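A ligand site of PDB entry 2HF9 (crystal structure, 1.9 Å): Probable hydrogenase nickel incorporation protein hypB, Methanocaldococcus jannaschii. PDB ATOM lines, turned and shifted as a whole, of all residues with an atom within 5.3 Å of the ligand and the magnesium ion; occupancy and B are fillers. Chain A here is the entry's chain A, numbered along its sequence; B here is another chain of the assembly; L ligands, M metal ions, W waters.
N of Thr 52 lies within hydrogen-bond range of O6 of the ligand, 3.5 Å away.
N of Leu 205 is in hydrogen-bond range of O13 of the ligand (2.7 Å).
The side-chain carboxylate (OD1) of Asp 175 sits at hydrogen-bond distance from a nitrogen (N3) of the ligand (2.7 Å).
An oxygen (O2) of the ligand is in hydrogen-bond range of the side-chain amino group of Lys 158 of chain B, at 2.8 Å.
The guanidinium group of Arg 83 lies within salt-bridge range of an oxygen (O7) of the ligand (2.9 Å).
The backbone NH of Leu 53 lies within hydrogen-bond range of an oxygen (O6) of the ligand, 2.9 Å away.
The side-chain amide oxygen (OD1) of Asn 172 sits close to a nitrogen (N2) of the ligand (2.9 Å).
The backbone NH (N) of Gly 50 lies within hydrogen-bond range of an oxygen (O4) of the ligand (2.9 Å).
O4 of the ligand lies within hydrogen-bond range of N of Lys 51, at 3.0 Å.
The side-chain amino group of Lys 51 is in salt-bridge range of an oxygen (O4) of the ligand.
O of Ala 179 of chain B is in hydrogen-bond range of N4 of the ligand (3.0 Å).
The backbone carbonyl oxygen of Val 180 of chain B lies within hydrogen-bond range of an oxygen (O11) of the ligand (3.0 Å).
O1 of the ligand sits close to N of Gly 48 (3.2 Å).
The backbone NH of Ser 49 lies within hydrogen-bond range of an oxygen (O4) of the ligand, 3.2 Å away.
N of Lys 173 sits close to O13 of the ligand.
Merely in contact with the ligand: Ile 47 (3.8 Å), Leu 176 (3.5 Å), Ser 204 (3.5 Å), Lys 206 (3.5 Å), Thr 150 of chain B (3.9 Å), Glu 151 of chain B (3.8 Å) and Gly 152 of chain B (3.8 Å).
Hydrophobic or aromatic side chains within 4 Å of the ligand: Leu 53, Leu 176, Leu 205 and Val 180 of chain B.
Within 4 Å of the ligand: Ile 47, Gly 48, Ser 49, Gly 50, Lys 51, Thr 52, Leu 53, Asp 80, Arg 83, Glu 125, Asn 172, Lys 173, Asp 175, Leu 176, Ser 204, Leu 205, Lys 206, Thr 150 of chain B, Glu 151 of chain B, Gly 152 of chain B, Lys 158 of chain B, Ala 179 of chain B and Val 180 of chain B.
Along chain A the residues within 4 Å of the ligand span positions 47 to 206.
The nearest printed residue that does not touch the ligand is Ala 46 (4.04 Å).
The backbone NH (N) of Leu 205 lies close to the side-chain amide nitrogen (ND2) of Asn 172 (3.4 Å).
OD1 of Asp 175 sits at hydrogen-bond distance from OG of Ser 204.
The side-chain amide oxygen (OD1) of Asn 172 sits close to the backbone carbonyl oxygen (O) of Ser 49 (3.0 Å).
ND2 of Asn 172 lies close to O of Leu 203 (3.3 Å).
The backbone carbonyl oxygen (O) of Ala 46 lies within hydrogen-bond range of the side-chain amino group (NZ) of Lys 51 (3.1 Å).
The backbone carbonyl oxygen of Gly 48 sits at hydrogen-bond distance from the side-chain amino group of Lys 173 (2.7 Å).
NZ of Lys 173 is in hydrogen-bond range of O of Thr 150 of chain B (2.7 Å).
The backbone NH (N) of Lys 173 is in hydrogen-bond range of the backbone carbonyl oxygen (O) of Leu 203, 3.0 Å away.
The magnesium ion is bound by an oxygen (O3) of the ligand, an oxygen (O5) of the ligand, water W6, the side-chain hydroxyl (OG1) of Thr 52, the side-chain carboxylate (OD2) of Asp 80 and the side-chain carboxylate (OE2) of Glu 125.
Lys 158 of chain B touches the magnesium ion (NZ to MG, 3.999 Å).
Within 4 Å of the magnesium ion: Thr 52, Asp 80, Glu 125 and Lys 158 of chain B.
Water W6 lies within hydrogen-bond range of OD1 of Asp 80 (2.7 Å), O7 of the ligand (2.7 Å), NZ of Lys 158 of chain B (2.8 Å) and NH1 of Arg 83 (3.3 Å).
Water W3 bridges N of Asp 153 of chain B (2.9 Å) and O11 of the ligand (2.9 Å).
Water W1 bridges O12 of the ligand (2.9 Å) and NH2 of Arg 83 (3.3 Å).
Water W4 lies within hydrogen-bond range of OD2 of Asp 74 (2.7 Å), NE2 of His 159 of chain B (2.9 Å) and O2 of the ligand (3.2 Å).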
ATOM      1  N   ALA A  46     -14.217 -29.058  10.515  1.00  0.00           N
ATOM      2  CA  ALA A  46     -13.370 -29.257   9.338  1.00  0.00           C
ATOM      3  C   ALA A  46     -12.536 -27.998   9.092  1.00  0.00           C
ATOM      4  O   ALA A  46     -12.643 -27.010   9.835  1.00  0.00           O
ATOM      5  CB  ALA A  46     -14.235 -29.571   8.126  1.00  0.00           C
ATOM      6  N   ILE A  47     -11.682 -28.021   8.070  1.00  0.00           N
ATOM      7  CA  ILE A  47     -10.875 -26.839   7.751  1.00  0.00           C
ATOM      8  C   ILE A  47     -11.779 -25.738   7.207  1.00  0.00           C
ATOM      9  O   ILE A  47     -12.509 -25.946   6.231  1.00  0.00           O
ATOM     10  CB  ILE A  47      -9.764 -27.151   6.725  1.00  0.00           C
ATOM     11  CG1 ILE A  47      -8.793 -28.216   7.244  1.00  0.00           C
ATOM     12  CG2 ILE A  47      -9.023 -25.866   6.331  1.00  0.00           C
ATOM     13  CD1 ILE A  47      -7.726 -27.712   8.215  1.00  0.00           C
ATOM     14  N   GLY A  48     -11.745 -24.575   7.862  1.00  0.00           N
ATOM     15  CA  GLY A  48     -12.463 -23.393   7.415  1.00  0.00           C
ATOM     16  C   GLY A  48     -13.979 -23.434   7.567  1.00  0.00           C
ATOM     17  O   GLY A  48     -14.679 -22.671   6.901  1.00  0.00           O
ATOM     18  N   SER A  49     -14.468 -24.307   8.444  1.00  0.00           N
ATOM     19  CA  SER A  49     -15.916 -24.453   8.662  1.00  0.00           C
ATOM     20  C   SER A  49     -16.560 -23.177   9.230  1.00  0.00           C
ATOM     21  O   SER A  49     -17.748 -22.921   9.006  1.00  0.00           O
ATOM     22  CB  SER A  49     -16.204 -25.629   9.591  1.00  0.00           C
ATOM     23  OG  SER A  49     -15.838 -26.854   8.987  1.00  0.00           O
ATOM     24  N   GLY A  50     -15.790 -22.402   9.989  1.00  0.00           N
ATOM     25  CA  GLY A  50     -16.273 -21.152  10.567  1.00  0.00           C
ATOM     26  C   GLY A  50     -16.099 -21.031  12.079  1.00  0.00           C
ATOM     27  O   GLY A  50     -16.765 -20.200  12.699  1.00  0.00           O
ATOM     28  N   LYS A  51     -15.210 -21.828  12.659  1.00  0.00           N
ATOM     29  CA  LYS A  51     -14.985 -21.853  14.109  1.00  0.00           C
ATOM     30  C   LYS A  51     -14.596 -20.488  14.663  1.00  0.00           C
ATOM     31  O   LYS A  51     -15.164 -20.014  15.643  1.00  0.00           O
ATOM     32  CB  LYS A  51     -13.905 -22.887  14.499  1.00  0.00           C
ATOM     33  CG  LYS A  51     -14.190 -24.325  14.084  1.00  0.00           C
ATOM     34  CD  LYS A  51     -13.097 -25.296  14.598  1.00  0.00           C
ATOM     35  CE  LYS A  51     -11.770 -25.172  13.842  1.00  0.00           C
ATOM     36  NZ  LYS A  51     -11.927 -25.327  12.375  1.00  0.00           N
ATOM     37  N   THR A  52     -13.609 -19.852  14.023  1.00  0.00           N
ATOM     38  CA  THR A  52     -13.119 -18.563  14.509  1.00  0.00           C
ATOM     39  C   THR A  52     -14.184 -17.473  14.373  1.00  0.00           C
ATOM     40  O   THR A  52     -14.415 -16.728  15.320  1.00  0.00           O
ATOM     41  CB  THR A  52     -11.820 -18.145  13.819  1.00  0.00           C
ATOM     42  OG1 THR A  52     -10.831 -19.148  14.041  1.00  0.00           O
ATOM     43  CG2 THR A  52     -11.305 -16.814  14.393  1.00  0.00           C
ATOM     44  N   LEU A  53     -14.823 -17.400  13.216  1.00  0.00           N
ATOM     45  CA  LEU A  53     -15.895 -16.427  13.002  1.00  0.00           C
ATOM     46  C   LEU A  53     -17.027 -16.610  14.024  1.00  0.00           C
ATOM     47  O   LEU A  53     -17.566 -15.627  14.522  1.00  0.00           O
ATOM     48  CB  LEU A  53     -16.420 -16.471  11.573  1.00  0.00           C
ATOM     49  CG  LEU A  53     -17.325 -15.315  11.127  1.00  0.00           C
ATOM     50  CD1 LEU A  53     -16.715 -13.940  11.415  1.00  0.00           C
ATOM     51  CD2 LEU A  53     -17.650 -15.450   9.648  1.00  0.00           C
ATOM     52  N   LEU A  54     -17.374 -17.859  14.318  1.00  0.00           N
ATOM     53  CA  LEU A  54     -18.377 -18.157  15.344  1.00  0.00           C
ATOM     54  C   LEU A  54     -17.929 -17.673  16.718  1.00  0.00           C
ATOM     55  O   LEU A  54     -18.704 -17.028  17.440  1.00  0.00           O
ATOM     56  CB  LEU A  54     -18.690 -19.658  15.394  1.00  0.00           C
ATOM     57  CG  LEU A  54     -19.704 -20.132  16.448  1.00  0.00           C
ATOM     58  CD1 LEU A  54     -21.058 -19.441  16.300  1.00  0.00           C
ATOM     59  CD2 LEU A  54     -19.862 -21.655  16.408  1.00  0.00           C
ATOM     60  N   ASP A  74      -3.600 -24.194  16.616  1.00  0.00           N
ATOM     61  CA  ASP A  74      -3.404 -24.533  15.204  1.00  0.00           C
ATOM     62  C   ASP A  74      -1.912 -24.605  14.922  1.00  0.00           C
ATOM     63  O   ASP A  74      -1.109 -24.243  15.779  1.00  0.00           O
ATOM     64  CB  ASP A  74      -4.079 -23.516  14.283  1.00  0.00           C
ATOM     65  CG  ASP A  74      -4.331 -24.045  12.882  1.00  0.00           C
ATOM     66  OD1 ASP A  74      -4.179 -25.264  12.630  1.00  0.00           O
ATOM     67  OD2 ASP A  74      -4.682 -23.238  12.000  1.00  0.00           O
ATOM     68  N   ASP A  80      -5.569 -16.994  14.266  1.00  0.00           N
ATOM     69  CA  ASP A  80      -6.841 -16.980  14.984  1.00  0.00           C
ATOM     70  C   ASP A  80      -6.752 -16.319  16.356  1.00  0.00           C
ATOM     71  O   ASP A  80      -7.723 -15.709  16.807  1.00  0.00           O
ATOM     72  CB  ASP A  80      -7.393 -18.395  15.104  1.00  0.00           C
ATOM     73  CG  ASP A  80      -7.808 -18.962  13.757  1.00  0.00           C
ATOM     74  OD1 ASP A  80      -7.791 -18.225  12.754  1.00  0.00           O
ATOM     75  OD2 ASP A  80      -8.162 -20.156  13.715  1.00  0.00           O
ATOM     76  N   ARG A  83      -7.162 -12.636  15.761  1.00  0.00           N
ATOM     77  CA  ARG A  83      -8.577 -12.375  15.496  1.00  0.00           C
ATOM     78  C   ARG A  83      -9.404 -12.297  16.777  1.00  0.00           C
ATOM     79  O   ARG A  83     -10.196 -11.376  16.945  1.00  0.00           O
ATOM     80  CB  ARG A  83      -9.158 -13.410  14.520  1.00  0.00           C
ATOM     81  CG  ARG A  83      -8.909 -13.079  13.048  1.00  0.00           C
ATOM     82  CD  ARG A  83      -9.266 -14.228  12.110  1.00  0.00           C
ATOM     83  NE  ARG A  83     -10.709 -14.430  11.984  1.00  0.00           N
ATOM     84  CZ  ARG A  83     -11.271 -15.371  11.224  1.00  0.00           C
ATOM     85  NH1 ARG A  83     -10.524 -16.217  10.529  1.00  0.00           N
ATOM     86  NH2 ARG A  83     -12.597 -15.482  11.178  1.00  0.00           N
ATOM     87  N   GLU A 125     -10.631 -23.214  20.509  1.00  0.00           N
ATOM     88  CA  GLU A 125     -10.669 -23.620  19.110  1.00  0.00           C
ATOM     89  C   GLU A 125      -9.678 -24.737  18.856  1.00  0.00           C
ATOM     90  O   GLU A 125      -8.461 -24.531  18.877  1.00  0.00           O
ATOM     91  CB  GLU A 125     -10.416 -22.456  18.148  1.00  0.00           C
ATOM     92  CG  GLU A 125     -10.600 -22.873  16.686  1.00  0.00           C
ATOM     93  CD  GLU A 125     -10.632 -21.711  15.727  1.00  0.00           C
ATOM     94  OE1 GLU A 125     -10.921 -20.584  16.162  1.00  0.00           O
ATOM     95  OE2 GLU A 125     -10.364 -21.922  14.524  1.00  0.00           O
ATOM     96  N   GLY A 128      -8.423 -27.920  13.044  1.00  0.00           N
ATOM     97  CA  GLY A 128      -9.404 -28.286  12.015  1.00  0.00           C
ATOM     98  C   GLY A 128      -9.177 -29.682  11.477  1.00  0.00           C
ATOM     99  O   GLY A 128      -8.264 -29.905  10.675  1.00  0.00           O
ATOM    100  N   ASN A 172     -22.988 -24.747   9.259  1.00  0.00           N
ATOM    101  CA  ASN A 172     -22.712 -23.357   8.956  1.00  0.00           C
ATOM    102  C   ASN A 172     -22.710 -23.096   7.450  1.00  0.00           C
ATOM    103  O   ASN A 172     -22.767 -24.041   6.650  1.00  0.00           O
ATOM    104  CB  ASN A 172     -21.364 -22.934   9.592  1.00  0.00           C
ATOM    105  CG  ASN A 172     -21.112 -21.437   9.541  1.00  0.00           C
ATOM    106  OD1 ASN A 172     -19.979 -20.992   9.326  1.00  0.00           O
ATOM    107  ND2 ASN A 172     -22.167 -20.648   9.734  1.00  0.00           N
ATOM    108  N   LYS A 173     -22.664 -21.820   7.073  1.00  0.00           N
ATOM    109  CA  LYS A 173     -22.646 -21.362   5.666  1.00  0.00           C
ATOM    110  C   LYS A 173     -23.905 -21.780   4.901  1.00  0.00           C
ATOM    111  O   LYS A 173     -23.838 -22.120   3.723  1.00  0.00           O
ATOM    112  CB  LYS A 173     -21.387 -21.846   4.931  1.00  0.00           C
ATOM    113  CG  LYS A 173     -20.066 -21.404   5.563  1.00  0.00           C
ATOM    114  CD  LYS A 173     -18.874 -21.838   4.719  1.00  0.00           C
ATOM    115  CE  LYS A 173     -17.597 -21.786   5.536  1.00  0.00           C
ATOM    116  NZ  LYS A 173     -16.562 -22.723   4.974  1.00  0.00           N
ATOM    117  N   ILE A 174     -25.058 -21.735   5.560  1.00  0.00           N
ATOM    118  CA  ILE A 174     -26.315 -22.119   4.898  1.00  0.00           C
ATOM    119  C   ILE A 174     -26.651 -21.183   3.728  1.00  0.00           C
ATOM    120  O   ILE A 174     -27.391 -21.562   2.822  1.00  0.00           O
ATOM    121  CB  ILE A 174     -27.523 -22.259   5.873  1.00  0.00           C
ATOM    122  CG1 ILE A 174     -27.859 -20.934   6.568  1.00  0.00           C
ATOM    123  CG2 ILE A 174     -27.269 -23.419   6.870  1.00  0.00           C
ATOM    124  CD1 ILE A 174     -29.178 -20.946   7.360  1.00  0.00           C
ATOM    125  N   ASP A 175     -26.073 -19.987   3.744  1.00  0.00           N
ATOM    126  CA  ASP A 175     -26.225 -19.028   2.660  1.00  0.00           C
ATOM    127  C   ASP A 175     -25.559 -19.486   1.356  1.00  0.00           C
ATOM    128  O   ASP A 175     -25.847 -18.950   0.287  1.00  0.00           O
ATOM    129  CB  ASP A 175     -25.720 -17.642   3.079  1.00  0.00           C
ATOM    130  CG  ASP A 175     -24.251 -17.635   3.489  1.00  0.00           C
ATOM    131  OD1 ASP A 175     -23.908 -18.179   4.568  1.00  0.00           O
ATOM    132  OD2 ASP A 175     -23.442 -17.069   2.732  1.00  0.00           O
ATOM    133  N   LEU A 176     -24.694 -20.505   1.438  1.00  0.00           N
ATOM    134  CA  LEU A 176     -23.953 -20.995   0.265  1.00  0.00           C
ATOM    135  C   LEU A 176     -24.397 -22.373  -0.231  1.00  0.00           C
ATOM    136  O   LEU A 176     -23.793 -22.925  -1.151  1.00  0.00           O
ATOM    137  CB  LEU A 176     -22.449 -21.021   0.574  1.00  0.00           C
ATOM    138  CG  LEU A 176     -21.815 -19.730   1.102  1.00  0.00           C
ATOM    139  CD1 LEU A 176     -20.369 -19.967   1.493  1.00  0.00           C
ATOM    140  CD2 LEU A 176     -21.913 -18.614   0.085  1.00  0.00           C
ATOM    141  N   LEU A 203     -26.964 -22.585  10.483  1.00  0.00           N
ATOM    142  CA  LEU A 203     -26.369 -21.278  10.724  1.00  0.00           C
ATOM    143  C   LEU A 203     -25.787 -20.630   9.480  1.00  0.00           C
ATOM    144  O   LEU A 203     -25.229 -21.305   8.619  1.00  0.00           O
ATOM    145  CB  LEU A 203     -25.261 -21.397  11.802  1.00  0.00           C
ATOM    146  CG  LEU A 203     -24.511 -20.124  12.224  1.00  0.00           C
ATOM    147  CD1 LEU A 203     -25.421 -19.140  12.932  1.00  0.00           C
ATOM    148  CD2 LEU A 203     -23.300 -20.459  13.087  1.00  0.00           C
ATOM    149  N   SER A 204     -25.943 -19.313   9.399  1.00  0.00           N
ATOM    150  CA  SER A 204     -25.116 -18.505   8.518  1.00  0.00           C
ATOM    151  C   SER A 204     -24.497 -17.393   9.343  1.00  0.00           C
ATOM    152  O   SER A 204     -25.224 -16.571   9.920  1.00  0.00           O
ATOM    153  CB  SER A 204     -25.923 -17.912   7.367  1.00  0.00           C
ATOM    154  OG  SER A 204     -25.119 -16.988   6.641  1.00  0.00           O
ATOM    155  N   LEU A 205     -23.173 -17.367   9.404  1.00  0.00           N
ATOM    156  CA  LEU A 205     -22.468 -16.272  10.080  1.00  0.00           C
ATOM    157  C   LEU A 205     -22.369 -15.021   9.207  1.00  0.00           C
ATOM    158  O   LEU A 205     -21.840 -13.997   9.648  1.00  0.00           O
ATOM    159  CB  LEU A 205     -21.094 -16.739  10.562  1.00  0.00           C
ATOM    160  CG  LEU A 205     -21.150 -17.708  11.745  1.00  0.00           C
ATOM    161  CD1 LEU A 205     -19.822 -18.425  11.932  1.00  0.00           C
ATOM    162  CD2 LEU A 205     -21.582 -16.988  13.044  1.00  0.00           C
ATOM    163  N   LYS A 206     -22.856 -15.121   7.976  1.00  0.00           N
ATOM    164  CA  LYS A 206     -22.955 -13.969   7.071  1.00  0.00           C
ATOM    165  C   LYS A 206     -24.282 -13.224   7.301  1.00  0.00           C
ATOM    166  O   LYS A 206     -24.279 -12.023   7.559  1.00  0.00           O
ATOM    167  CB  LYS A 206     -22.817 -14.419   5.614  1.00  0.00           C
ATOM    168  CG  LYS A 206     -22.794 -13.289   4.585  1.00  0.00           C
ATOM    169  CD  LYS A 206     -22.425 -13.841   3.210  1.00  0.00           C
ATOM    170  CE  LYS A 206     -22.084 -12.747   2.217  1.00  0.00           C
ATOM    171  NZ  LYS A 206     -21.504 -13.341   0.972  1.00  0.00           N
ATOM    172  N   THR B 150     -13.522 -21.615  -0.087  1.00  0.00           N
ATOM    173  CA  THR B 150     -14.513 -21.604   1.006  1.00  0.00           C
ATOM    174  C   THR B 150     -13.925 -21.982   2.372  1.00  0.00           C
ATOM    175  O   THR B 150     -14.573 -21.814   3.400  1.00  0.00           O
ATOM    176  CB  THR B 150     -15.764 -22.453   0.689  1.00  0.00           C
ATOM    177  OG1 THR B 150     -15.384 -23.807   0.362  1.00  0.00           O
ATOM    178  CG2 THR B 150     -16.541 -21.845  -0.475  1.00  0.00           C
ATOM    179  N   GLU B 151     -12.686 -22.483   2.368  1.00  0.00           N
ATOM    180  CA  GLU B 151     -11.957 -22.757   3.604  1.00  0.00           C
ATOM    181  C   GLU B 151     -11.331 -21.477   4.207  1.00  0.00           C
ATOM    182  O   GLU B 151     -10.822 -21.489   5.326  1.00  0.00           O
ATOM    183  CB  GLU B 151     -10.890 -23.822   3.348  1.00  0.00           C
ATOM    184  CG  GLU B 151     -11.468 -25.197   3.040  1.00  0.00           C
ATOM    185  CD  GLU B 151     -10.690 -25.957   1.962  1.00  0.00           C
ATOM    186  OE1 GLU B 151      -9.470 -25.742   1.820  1.00  0.00           O
ATOM    187  OE2 GLU B 151     -11.310 -26.789   1.248  1.00  0.00           O
ATOM    188  N   GLY B 152     -11.404 -20.385   3.451  1.00  0.00           N
ATOM    189  CA  GLY B 152     -10.774 -19.121   3.864  1.00  0.00           C
ATOM    190  C   GLY B 152      -9.430 -18.942   3.180  1.00  0.00           C
ATOM    191  O   GLY B 152      -8.731 -19.931   2.915  1.00  0.00           O
ATOM    192  N   ASP B 153      -9.060 -17.694   2.905  1.00  0.00           N
ATOM    193  CA  ASP B 153      -7.853 -17.425   2.111  1.00  0.00           C
ATOM    194  C   ASP B 153      -6.539 -17.506   2.890  1.00  0.00           C
ATOM    195  O   ASP B 153      -5.472 -17.196   2.350  1.00  0.00           O
ATOM    196  CB  ASP B 153      -7.968 -16.105   1.320  1.00  0.00           C
ATOM    197  CG  ASP B 153      -8.194 -14.892   2.205  1.00  0.00           C
ATOM    198  OD1 ASP B 153      -7.940 -14.955   3.434  1.00  0.00           O
ATOM    199  OD2 ASP B 153      -8.618 -13.858   1.666  1.00  0.00           O
ATOM    200  N   LYS B 158      -1.564 -21.179   6.416  1.00  0.00           N
ATOM    201  CA  LYS B 158      -1.756 -21.889   7.697  1.00  0.00           C
ATOM    202  C   LYS B 158      -1.243 -23.336   7.684  1.00  0.00           C
ATOM    203  O   LYS B 158      -1.099 -23.949   8.746  1.00  0.00           O
ATOM    204  CB  LYS B 158      -3.223 -21.895   8.087  1.00  0.00           C
ATOM    205  CG  LYS B 158      -3.730 -20.604   8.682  1.00  0.00           C
ATOM    206  CD  LYS B 158      -5.228 -20.694   8.926  1.00  0.00           C
ATOM    207  CE  LYS B 158      -5.713 -19.550   9.771  1.00  0.00           C
ATOM    208  NZ  LYS B 158      -7.100 -19.817  10.261  1.00  0.00           N
ATOM    209  N   HIS B 159      -0.988 -23.882   6.504  1.00  0.00           N
ATOM    210  CA  HIS B 159      -0.571 -25.275   6.382  1.00  0.00           C
ATOM    211  C   HIS B 159       0.603 -25.459   5.431  1.00  0.00           C
ATOM    212  O   HIS B 159       0.510 -26.210   4.453  1.00  0.00           O
ATOM    213  CB  HIS B 159      -1.760 -26.160   5.976  1.00  0.00           C
ATOM    214  CG  HIS B 159      -2.960 -25.988   6.854  1.00  0.00           C
ATOM    215  ND1 HIS B 159      -3.950 -25.065   6.571  1.00  0.00           N
ATOM    216  CD2 HIS B 159      -3.313 -26.576   8.020  1.00  0.00           C
ATOM    217  CE1 HIS B 159      -4.873 -25.118   7.527  1.00  0.00           C
ATOM    218  NE2 HIS B 159      -4.498 -26.023   8.413  1.00  0.00           N
ATOM    219  N   ALA B 179     -18.263 -14.763  -2.182  1.00  0.00           N
ATOM    220  CA  ALA B 179     -19.269 -15.100  -1.183  1.00  0.00           C
ATOM    221  C   ALA B 179     -18.686 -15.365   0.215  1.00  0.00           C
ATOM    222  O   ALA B 179     -19.338 -15.104   1.225  1.00  0.00           O
ATOM    223  CB  ALA B 179     -20.104 -16.284  -1.652  1.00  0.00           C
ATOM    224  N   VAL B 180     -17.448 -15.881   0.267  1.00  0.00           N
ATOM    225  CA  VAL B 180     -16.751 -16.093   1.546  1.00  0.00           C
ATOM    226  C   VAL B 180     -15.748 -14.983   1.875  1.00  0.00           C
ATOM    227  O   VAL B 180     -15.140 -14.995   2.955  1.00  0.00           O
ATOM    228  CB  VAL B 180     -16.025 -17.483   1.591  1.00  0.00           C
ATOM    229  CG1 VAL B 180     -17.028 -18.611   1.784  1.00  0.00           C
ATOM    230  CG2 VAL B 180     -15.177 -17.712   0.344  1.00  0.00           C
ATOM    231  N   GLY B 181     -15.572 -14.046   0.958  1.00  0.00           N
ATOM    232  CA  GLY B 181     -14.636 -12.942   1.145  1.00  0.00           C
ATOM    233  C   GLY B 181     -13.176 -13.334   0.921  1.00  0.00           C
ATOM    234  O   GLY B 181     -12.268 -12.597   1.315  1.00  0.00           O
ATOM    235  N   ALA B 182     -12.951 -14.493   0.307  1.00  0.00           N
ATOM    236  CA  ALA B 182     -11.595 -14.977   0.007  1.00  0.00           C
ATOM    237  C   ALA B 182     -10.914 -14.179  -1.109  1.00  0.00           C
ATOM    238  O   ALA B 182     -11.520 -13.904  -2.150  1.00  0.00           O
ATOM    239  CB  ALA B 182     -11.625 -16.444  -0.342  1.00  0.00           C
HETATM  240  P1  LIG L   1      -9.541 -22.733  10.477  1.00  0.00           P
HETATM  241  O1  LIG L   1     -10.929 -22.169   9.886  1.00  0.00           O
HETATM  242  S1  LIG L   1      -9.565 -24.460  10.437  1.00  0.00           S
HETATM  243  O2  LIG L   1      -8.431 -22.194   9.566  1.00  0.00           O
HETATM  244  O3  LIG L   1      -9.348 -22.205  11.912  1.00  0.00           O
HETATM  245  P2  LIG L   1     -12.209 -21.765  10.768  1.00  0.00           P
HETATM  246  O4  LIG L   1     -13.061 -22.964  10.943  1.00  0.00           O
HETATM  247  O5  LIG L   1     -11.867 -21.122  12.053  1.00  0.00           O
HETATM  248  P3  LIG L   1     -13.040 -19.206   9.661  1.00  0.00           P
HETATM  249  O6  LIG L   1     -13.778 -18.597  10.803  1.00  0.00           O
HETATM  250  O7  LIG L   1     -11.678 -18.646   9.520  1.00  0.00           O
HETATM  251  O8  LIG L   1     -13.024 -20.808   9.754  1.00  0.00           O
HETATM  252  O9  LIG L   1     -13.929 -19.016   8.338  1.00  0.00           O
HETATM  253  C1  LIG L   1     -13.509 -19.540   7.096  1.00  0.00           C
HETATM  254  C2  LIG L   1     -14.067 -18.692   5.958  1.00  0.00           C
HETATM  255  O10 LIG L   1     -15.465 -18.886   5.835  1.00  0.00           O
HETATM  256  C3  LIG L   1     -13.863 -17.207   6.162  1.00  0.00           C
HETATM  257  O11 LIG L   1     -13.551 -16.683   4.884  1.00  0.00           O
HETATM  258  C4  LIG L   1     -15.210 -16.698   6.623  1.00  0.00           C
HETATM  259  O12 LIG L   1     -15.460 -15.382   6.215  1.00  0.00           O
HETATM  260  C5  LIG L   1     -16.156 -17.660   5.920  1.00  0.00           C
HETATM  261  N1  LIG L   1     -17.435 -17.938   6.603  1.00  0.00           N
HETATM  262  C6  LIG L   1     -17.630 -18.455   7.857  1.00  0.00           C
HETATM  263  N2  LIG L   1     -18.966 -18.602   8.041  1.00  0.00           N
HETATM  264  C7  LIG L   1     -19.610 -18.222   6.914  1.00  0.00           C
HETATM  265  C8  LIG L   1     -20.950 -18.179   6.564  1.00  0.00           C
HETATM  266  O13 LIG L   1     -21.817 -18.536   7.359  1.00  0.00           O
HETATM  267  N3  LIG L   1     -21.310 -17.726   5.301  1.00  0.00           N
HETATM  268  C9  LIG L   1     -20.327 -17.323   4.400  1.00  0.00           C
HETATM  269  N4  LIG L   1     -20.675 -16.887   3.198  1.00  0.00           N
HETATM  270  N5  LIG L   1     -18.998 -17.370   4.757  1.00  0.00           N
HETATM  271  C10 LIG L   1     -18.649 -17.817   5.994  1.00  0.00           C
HETATM  272 MG    MG M   1     -10.043 -20.639  12.841  1.00  0.00          MG
HETATM  273  O   HOH W   1     -14.008 -14.185   8.455  1.00  0.00           O
HETATM  274  O   HOH W   2     -18.059 -14.288   4.941  1.00  0.00           O
HETATM  275  O   HOH W   3     -11.029 -15.774   3.766  1.00  0.00           O
HETATM  276  O   HOH W   4      -6.273 -24.445  10.132  1.00  0.00           O
HETATM  277  O   HOH W   5      -7.275 -22.884   7.188  1.00  0.00           O
HETATM  278  O   HOH W   6      -9.723 -19.372  11.269  1.00  0.00           O
